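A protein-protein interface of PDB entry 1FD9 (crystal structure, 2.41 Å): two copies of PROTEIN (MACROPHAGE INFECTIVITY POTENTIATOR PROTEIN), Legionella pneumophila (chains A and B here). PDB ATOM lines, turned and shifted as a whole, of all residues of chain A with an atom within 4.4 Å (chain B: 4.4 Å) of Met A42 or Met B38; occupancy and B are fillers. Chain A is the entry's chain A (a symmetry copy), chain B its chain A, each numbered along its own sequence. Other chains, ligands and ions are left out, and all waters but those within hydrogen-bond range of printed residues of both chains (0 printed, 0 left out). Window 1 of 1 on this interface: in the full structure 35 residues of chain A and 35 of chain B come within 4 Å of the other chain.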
ATOM      1  N   SER A  15     -28.648   2.638  24.052  1.00  0.00           N
ATOM      2  CA  SER A  15     -27.271   2.256  23.761  1.00  0.00           C
ATOM      3  C   SER A  15     -26.811   2.847  22.436  1.00  0.00           C
ATOM      4  O   SER A  15     -25.739   3.453  22.346  1.00  0.00           O
ATOM      5  CB  SER A  15     -27.142   0.734  23.720  1.00  0.00           C
ATOM      6  OG  SER A  15     -27.583   0.153  24.935  1.00  0.00           O
ATOM      7  N   TYR A  16     -27.636   2.678  21.409  1.00  0.00           N
ATOM      8  CA  TYR A  16     -27.297   3.191  20.093  1.00  0.00           C
ATOM      9  C   TYR A  16     -27.083   4.691  20.130  1.00  0.00           C
ATOM     10  O   TYR A  16     -26.081   5.210  19.627  1.00  0.00           O
ATOM     11  CB  TYR A  16     -28.408   2.891  19.086  1.00  0.00           C
ATOM     12  CG  TYR A  16     -28.078   3.411  17.700  1.00  0.00           C
ATOM     13  CD1 TYR A  16     -27.243   2.691  16.846  1.00  0.00           C
ATOM     14  CD2 TYR A  16     -28.543   4.652  17.271  1.00  0.00           C
ATOM     15  CE1 TYR A  16     -26.884   3.195  15.605  1.00  0.00           C
ATOM     16  CE2 TYR A  16     -28.181   5.166  16.036  1.00  0.00           C
ATOM     17  CZ  TYR A  16     -27.352   4.432  15.209  1.00  0.00           C
ATOM     18  OH  TYR A  16     -26.988   4.936  13.986  1.00  0.00           O
ATOM     19  N   ILE A  18     -26.339   6.776  22.571  1.00  0.00           N
ATOM     20  CA  ILE A  18     -25.113   7.163  23.268  1.00  0.00           C
ATOM     21  C   ILE A  18     -23.910   6.986  22.358  1.00  0.00           C
ATOM     22  O   ILE A  18     -23.106   7.902  22.202  1.00  0.00           O
ATOM     23  CB  ILE A  18     -24.878   6.310  24.541  1.00  0.00           C
ATOM     24  CG1 ILE A  18     -26.020   6.524  25.545  1.00  0.00           C
ATOM     25  CG2 ILE A  18     -23.534   6.670  25.157  1.00  0.00           C
ATOM     26  CD1 ILE A  18     -25.990   5.580  26.743  1.00  0.00           C
ATOM     27  N   GLY A  19     -23.790   5.800  21.766  1.00  0.00           N
ATOM     28  CA  GLY A  19     -22.674   5.519  20.878  1.00  0.00           C
ATOM     29  C   GLY A  19     -22.684   6.378  19.626  1.00  0.00           C
ATOM     30  O   GLY A  19     -21.630   6.773  19.107  1.00  0.00           O
ATOM     31  N   MET A  38     -12.311  -1.354  20.491  1.00  0.00           N
ATOM     32  CA  MET A  38     -12.905  -0.389  21.394  1.00  0.00           C
ATOM     33  C   MET A  38     -14.151  -0.955  22.045  1.00  0.00           C
ATOM     34  O   MET A  38     -14.453  -0.636  23.187  1.00  0.00           O
ATOM     35  CB  MET A  38     -13.267   0.896  20.651  1.00  0.00           C
ATOM     36  CG  MET A  38     -13.882   1.955  21.556  1.00  0.00           C
ATOM     37  SD  MET A  38     -14.201   3.510  20.716  1.00  0.00           S
ATOM     38  CE  MET A  38     -12.596   4.302  20.811  1.00  0.00           C
ATOM     39  N   ALA A  39     -14.889  -1.780  21.311  1.00  0.00           N
ATOM     40  CA  ALA A  39     -16.096  -2.382  21.859  1.00  0.00           C
ATOM     41  C   ALA A  39     -15.639  -3.474  22.811  1.00  0.00           C
ATOM     42  O   ALA A  39     -16.319  -3.809  23.789  1.00  0.00           O
ATOM     43  CB  ALA A  39     -16.936  -2.970  20.748  1.00  0.00           C
ATOM     44  N   LYS A  40     -14.464  -4.015  22.513  1.00  0.00           N
ATOM     45  CA  LYS A  40     -13.870  -5.068  23.317  1.00  0.00           C
ATOM     46  C   LYS A  40     -13.622  -4.579  24.732  1.00  0.00           C
ATOM     47  O   LYS A  40     -14.102  -5.175  25.693  1.00  0.00           O
ATOM     48  CB  LYS A  40     -12.548  -5.526  22.699  1.00  0.00           C
ATOM     49  CG  LYS A  40     -11.898  -6.677  23.448  1.00  0.00           C
ATOM     50  CD  LYS A  40     -12.873  -7.838  23.578  1.00  0.00           C
ATOM     51  CE  LYS A  40     -12.261  -9.007  24.318  1.00  0.00           C
ATOM     52  NZ  LYS A  40     -13.249 -10.108  24.434  1.00  0.00           N
ATOM     53  N   GLY A  41     -12.865  -3.491  24.853  1.00  0.00           N
ATOM     54  CA  GLY A  41     -12.560  -2.943  26.163  1.00  0.00           C
ATOM     55  C   GLY A  41     -13.793  -2.640  26.990  1.00  0.00           C
ATOM     56  O   GLY A  41     -13.820  -2.839  28.208  1.00  0.00           O
ATOM     57  N   MET A  42     -14.829  -2.160  26.323  1.00  0.00           N
ATOM     58  CA  MET A  42     -16.046  -1.825  27.020  1.00  0.00           C
ATOM     59  C   MET A  42     -16.610  -3.043  27.729  1.00  0.00           C
ATOM     60  O   MET A  42     -17.023  -2.951  28.887  1.00  0.00           O
ATOM     61  CB  MET A  42     -17.073  -1.254  26.045  1.00  0.00           C
ATOM     62  CG  MET A  42     -18.291  -0.649  26.729  1.00  0.00           C
ATOM     63  SD  MET A  42     -19.299   0.299  25.581  1.00  0.00           S
ATOM     64  CE  MET A  42     -18.109   1.651  25.152  1.00  0.00           C
ATOM     65  N   GLN A  43     -16.624  -4.186  27.046  1.00  0.00           N
ATOM     66  CA  GLN A  43     -17.154  -5.410  27.646  1.00  0.00           C
ATOM     67  C   GLN A  43     -16.273  -5.893  28.800  1.00  0.00           C
ATOM     68  O   GLN A  43     -16.784  -6.307  29.841  1.00  0.00           O
ATOM     69  CB  GLN A  43     -17.297  -6.518  26.596  1.00  0.00           C
ATOM     70  CG  GLN A  43     -17.997  -7.775  27.111  1.00  0.00           C
ATOM     71  N   ASP A  44     -14.955  -5.847  28.619  1.00  0.00           N
ATOM     72  CA  ASP A  44     -14.051  -6.266  29.686  1.00  0.00           C
ATOM     73  C   ASP A  44     -14.451  -5.490  30.936  1.00  0.00           C
ATOM     74  O   ASP A  44     -14.763  -6.068  31.981  1.00  0.00           O
ATOM     75  CB  ASP A  44     -12.593  -5.943  29.332  1.00  0.00           C
ATOM     76  CG  ASP A  44     -12.042  -6.834  28.235  1.00  0.00           C
ATOM     77  OD1 ASP A  44     -12.182  -8.067  28.345  1.00  0.00           O
ATOM     78  OD2 ASP A  44     -11.455  -6.311  27.269  1.00  0.00           O
ATOM     79  N   ALA A  45     -14.457  -4.169  30.799  1.00  0.00           N
ATOM     80  CA  ALA A  45     -14.806  -3.265  31.886  1.00  0.00           C
ATOM     81  C   ALA A  45     -16.104  -3.643  32.600  1.00  0.00           C
ATOM     82  O   ALA A  45     -16.106  -3.921  33.797  1.00  0.00           O
ATOM     83  CB  ALA A  45     -14.896  -1.835  31.350  1.00  0.00           C
ATOM     84  N   MET A  46     -17.207  -3.653  31.864  1.00  0.00           N
ATOM     85  CA  MET A  46     -18.498  -3.989  32.445  1.00  0.00           C
ATOM     86  C   MET A  46     -18.599  -5.391  33.043  1.00  0.00           C
ATOM     87  O   MET A  46     -19.276  -5.584  34.054  1.00  0.00           O
ATOM     88  CB  MET A  46     -19.612  -3.804  31.411  1.00  0.00           C
ATOM     89  CG  MET A  46     -19.977  -2.359  31.142  1.00  0.00           C
ATOM     90  SD  MET A  46     -21.574  -2.228  30.302  1.00  0.00           S
ATOM     91  CE  MET A  46     -21.015  -1.889  28.612  1.00  0.00           C
ATOM     92  N   GLY B  19     -11.912   2.788  24.770  1.00  0.00           N
ATOM     93  CA  GLY B  19     -13.136   2.067  25.079  1.00  0.00           C
ATOM     94  C   GLY B  19     -13.105   1.409  26.447  1.00  0.00           C
ATOM     95  O   GLY B  19     -14.125   1.324  27.145  1.00  0.00           O
ATOM     96  N   ALA B  20     -11.928   0.916  26.823  1.00  0.00           N
ATOM     97  CA  ALA B  20     -11.761   0.286  28.119  1.00  0.00           C
ATOM     98  C   ALA B  20     -12.062   1.394  29.124  1.00  0.00           C
ATOM     99  O   ALA B  20     -12.852   1.225  30.066  1.00  0.00           O
ATOM    100  CB  ALA B  20     -10.323  -0.216  28.271  1.00  0.00           C
ATOM    101  N   GLY B  23     -16.030   2.371  28.755  1.00  0.00           N
ATOM    102  CA  GLY B  23     -16.811   1.269  29.304  1.00  0.00           C
ATOM    103  C   GLY B  23     -16.831   1.097  30.818  1.00  0.00           C
ATOM    104  O   GLY B  23     -17.864   0.719  31.396  1.00  0.00           O
ATOM    105  N   PHE B  26     -19.154   4.062  32.506  1.00  0.00           N
ATOM    106  CA  PHE B  26     -20.574   3.764  32.359  1.00  0.00           C
ATOM    107  C   PHE B  26     -21.002   2.792  33.457  1.00  0.00           C
ATOM    108  O   PHE B  26     -21.773   3.137  34.351  1.00  0.00           O
ATOM    109  CB  PHE B  26     -20.849   3.107  30.999  1.00  0.00           C
ATOM    110  CG  PHE B  26     -20.434   3.937  29.810  1.00  0.00           C
ATOM    111  CD1 PHE B  26     -19.150   4.465  29.716  1.00  0.00           C
ATOM    112  CD2 PHE B  26     -21.317   4.141  28.752  1.00  0.00           C
ATOM    113  CE1 PHE B  26     -18.752   5.179  28.589  1.00  0.00           C
ATOM    114  CE2 PHE B  26     -20.927   4.854  27.621  1.00  0.00           C
ATOM    115  CZ  PHE B  26     -19.642   5.373  27.540  1.00  0.00           C
ATOM    116  N   VAL B  33     -26.207  -1.008  29.180  1.00  0.00           N
ATOM    117  CA  VAL B  33     -26.304  -0.974  27.720  1.00  0.00           C
ATOM    118  C   VAL B  33     -25.934  -2.275  27.007  1.00  0.00           C
ATOM    119  O   VAL B  33     -25.750  -3.321  27.634  1.00  0.00           O
ATOM    120  CB  VAL B  33     -25.386   0.155  27.132  1.00  0.00           C
ATOM    121  CG1 VAL B  33     -25.608   1.462  27.890  1.00  0.00           C
ATOM    122  CG2 VAL B  33     -23.907  -0.263  27.197  1.00  0.00           C
ATOM    123  N   ASN B  34     -25.841  -2.179  25.681  1.00  0.00           N
ATOM    124  CA  ASN B  34     -25.446  -3.286  24.813  1.00  0.00           C
ATOM    125  C   ASN B  34     -24.454  -2.666  23.823  1.00  0.00           C
ATOM    126  O   ASN B  34     -24.850  -2.008  22.865  1.00  0.00           O
ATOM    127  CB  ASN B  34     -26.665  -3.867  24.079  1.00  0.00           C
ATOM    128  CG  ASN B  34     -27.241  -2.917  23.040  1.00  0.00           C
ATOM    129  OD1 ASN B  34     -26.855  -2.943  21.867  1.00  0.00           O
ATOM    130  ND2 ASN B  34     -28.163  -2.065  23.469  1.00  0.00           N
ATOM    131  N   PRO B  35     -23.141  -2.841  24.069  1.00  0.00           N
ATOM    132  CA  PRO B  35     -22.091  -2.290  23.199  1.00  0.00           C
ATOM    133  C   PRO B  35     -22.194  -2.689  21.729  1.00  0.00           C
ATOM    134  O   PRO B  35     -21.352  -2.290  20.918  1.00  0.00           O
ATOM    135  CB  PRO B  35     -20.799  -2.800  23.844  1.00  0.00           C
ATOM    136  CG  PRO B  35     -21.157  -2.851  25.308  1.00  0.00           C
ATOM    137  CD  PRO B  35     -22.548  -3.474  25.264  1.00  0.00           C
ATOM    138  N   GLU B  36     -23.219  -3.470  21.389  1.00  0.00           N
ATOM    139  CA  GLU B  36     -23.402  -3.907  20.012  1.00  0.00           C
ATOM    140  C   GLU B  36     -24.139  -2.837  19.208  1.00  0.00           C
ATOM    141  O   GLU B  36     -23.704  -2.473  18.112  1.00  0.00           O
ATOM    142  CB  GLU B  36     -24.171  -5.229  19.974  1.00  0.00           C
ATOM    143  CG  GLU B  36     -24.154  -5.910  18.613  1.00  0.00           C
ATOM    144  N   ALA B  37     -25.253  -2.339  19.747  1.00  0.00           N
ATOM    145  CA  ALA B  37     -26.027  -1.285  19.081  1.00  0.00           C
ATOM    146  C   ALA B  37     -25.244   0.006  19.259  1.00  0.00           C
ATOM    147  O   ALA B  37     -25.342   0.934  18.451  1.00  0.00           O
ATOM    148  CB  ALA B  37     -27.406  -1.151  19.718  1.00  0.00           C
ATOM    149  N   MET B  38     -24.457   0.045  20.332  1.00  0.00           N
ATOM    150  CA  MET B  38     -23.635   1.195  20.650  1.00  0.00           C
ATOM    151  C   MET B  38     -22.441   1.279  19.721  1.00  0.00           C
ATOM    152  O   MET B  38     -21.988   2.367  19.391  1.00  0.00           O
ATOM    153  CB  MET B  38     -23.142   1.126  22.095  1.00  0.00           C
ATOM    154  CG  MET B  38     -22.284   2.320  22.490  1.00  0.00           C
ATOM    155  SD  MET B  38     -21.799   2.306  24.220  1.00  0.00           S
ATOM    156  CE  MET B  38     -23.241   3.030  25.000  1.00  0.00           C
ATOM    157  N   ALA B  39     -21.916   0.129  19.315  1.00  0.00           N
ATOM    158  CA  ALA B  39     -20.775   0.113  18.410  1.00  0.00           C
ATOM    159  C   ALA B  39     -21.311   0.472  17.034  1.00  0.00           C
ATOM    160  O   ALA B  39     -20.606   1.039  16.190  1.00  0.00           O
ATOM    161  CB  ALA B  39     -20.147  -1.262  18.388  1.00  0.00           C
ATOM    162  N   LYS B  40     -22.580   0.141  16.829  1.00  0.00           N
ATOM    163  CA  LYS B  40     -23.258   0.413  15.574  1.00  0.00           C
ATOM    164  C   LYS B  40     -23.293   1.906  15.303  1.00  0.00           C
ATOM    165  O   LYS B  40     -22.827   2.364  14.262  1.00  0.00           O
ATOM    166  CB  LYS B  40     -24.688  -0.129  15.615  1.00  0.00           C
ATOM    167  CG  LYS B  40     -25.442   0.057  14.309  1.00  0.00           C
ATOM    168  CD  LYS B  40     -24.658  -0.553  13.156  1.00  0.00           C
ATOM    169  CE  LYS B  40     -25.378  -0.389  11.836  1.00  0.00           C
ATOM    170  NZ  LYS B  40     -24.573  -0.984  10.741  1.00  0.00           N
ATOM    171  N   GLY B  41     -23.852   2.661  16.246  1.00  0.00           N
ATOM    172  CA  GLY B  41     -23.943   4.102  16.084  1.00  0.00           C
ATOM    173  C   GLY B  41     -22.606   4.761  15.813  1.00  0.00           C
ATOM    174  O   GLY B  41     -22.498   5.706  15.026  1.00  0.00           O
ATOM    175  N   MET B  42     -21.572   4.257  16.466  1.00  0.00           N
ATOM    176  CA  MET B  42     -20.258   4.823  16.289  1.00  0.00           C
ATOM    177  C   MET B  42     -19.833   4.748  14.833  1.00  0.00           C
ATOM    178  O   MET B  42     -19.305   5.722  14.291  1.00  0.00           O
ATOM    179  CB  MET B  42     -19.247   4.100  17.176  1.00  0.00           C
ATOM    180  CG  MET B  42     -17.891   4.787  17.238  1.00  0.00           C
ATOM    181  SD  MET B  42     -16.854   4.102  18.538  1.00  0.00           S
ATOM    182  CE  MET B  42     -17.846   4.582  20.025  1.00  0.00           C
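Among the printed residues, merely in contact across the chains: Ser A15 with Val B33 (3.1 Å), Ser A15 with Met B38 (3.5 Å), Tyr A16 with Ala B37 (3.0 Å), Tyr A16 with Lys B40 (3.7 Å), Tyr A16 with Gly B41 (3.1 Å), Ile A18 with Met B38 (3.7 Å), Gly A19 with Met B38 (3.6 Å), Gly A19 with Gly B41 (3.98 Å), Gly A19 with Met B42 (3.6 Å), Met A38 with Gly B19 (3.6 Å), Gly A41 with Gly B19 (3.98 Å), Gly A41 with Ala B20 (3.7 Å), Met A42 with Gly B19 (3.6 Å), Met A42 with Gly B23 (3.5 Å), Met A42 with Pro B35 (3.7 Å), Ala A45 with Ala B20 (3.9 Å), Ala A45 with Gly B23 (3.6 Å), Met A46 with Gly B23 (3.7 Å), Met A46 with Val B33 (3.6 Å) and Met A46 with Pro B35 (3.4 Å).
Gly A19 touches Met B38, and with the chains exchanged Met A38 touches Gly B19.
Gly A19 touches Gly B41, and with the chains exchanged Gly A41 touches Gly B19.
Gly A19 touches Met B42, and with the chains exchanged Met A42 touches Gly B19.
Met A38 touches Met B42, and with the chains exchanged Met A42 touches Met B38.
Positions printed for both chains: 19, 38, 39, 40, 41 and 42.
The side-chain sulfur (SD) of Met B38 lies close to the side-chain sulfur (SD) of Met A42, 3.5 Å away.
SD of Met A38 lies close to SD of Met B42, 3.5 Å away.
ND2 of Asn B34 sits at hydrogen-bond distance from OG of Ser A15 (2.7 Å).
OD1 of Asn B34 sits at hydrogen-bond distance from N of Ala B37, at 2.7 Å.
Hydrophobic or aromatic side chains of chain B that line the printed part of chain A: Val B33, Pro B35, Met B38 and Met B42.
Along chain B the printed residues that touch a printed residue of chain A span positions 19 to 42.
Of the 13 printed residues of chain A, 9 touch a printed residue of chain B.
Printed residues of chain A that touch a printed residue of chain B: Ser A15, Tyr A16, Ile A18, Gly A19, Met A38, Gly A41, Met A42, Ala A45 and Met A46.
Among the printed residues, no Asp or Glu carboxylate lies within 4 Å of a Lys or Arg side-chain nitrogen of the other chain.
Met B38 touches just these residues of chain A: Ser A15 (3.5 Å), Ile A18 (3.7 Å), Gly A19 (3.6 Å) and Met A42 (3.5 Å).
Of the printed residues of chain B, Gly A41 touches Gly B19 (3.98 Å) and Ala B20 (3.7 Å).
Printed residues of chain A within 4 Å of Pro B35: Met A42 (3.7 Å) and Met A46 (3.4 Å).
Glu B36 touches none of the printed residues of chain A.
The nearest residue of chain B that does not touch Met A42 is Ala B20 (4.3 Å).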
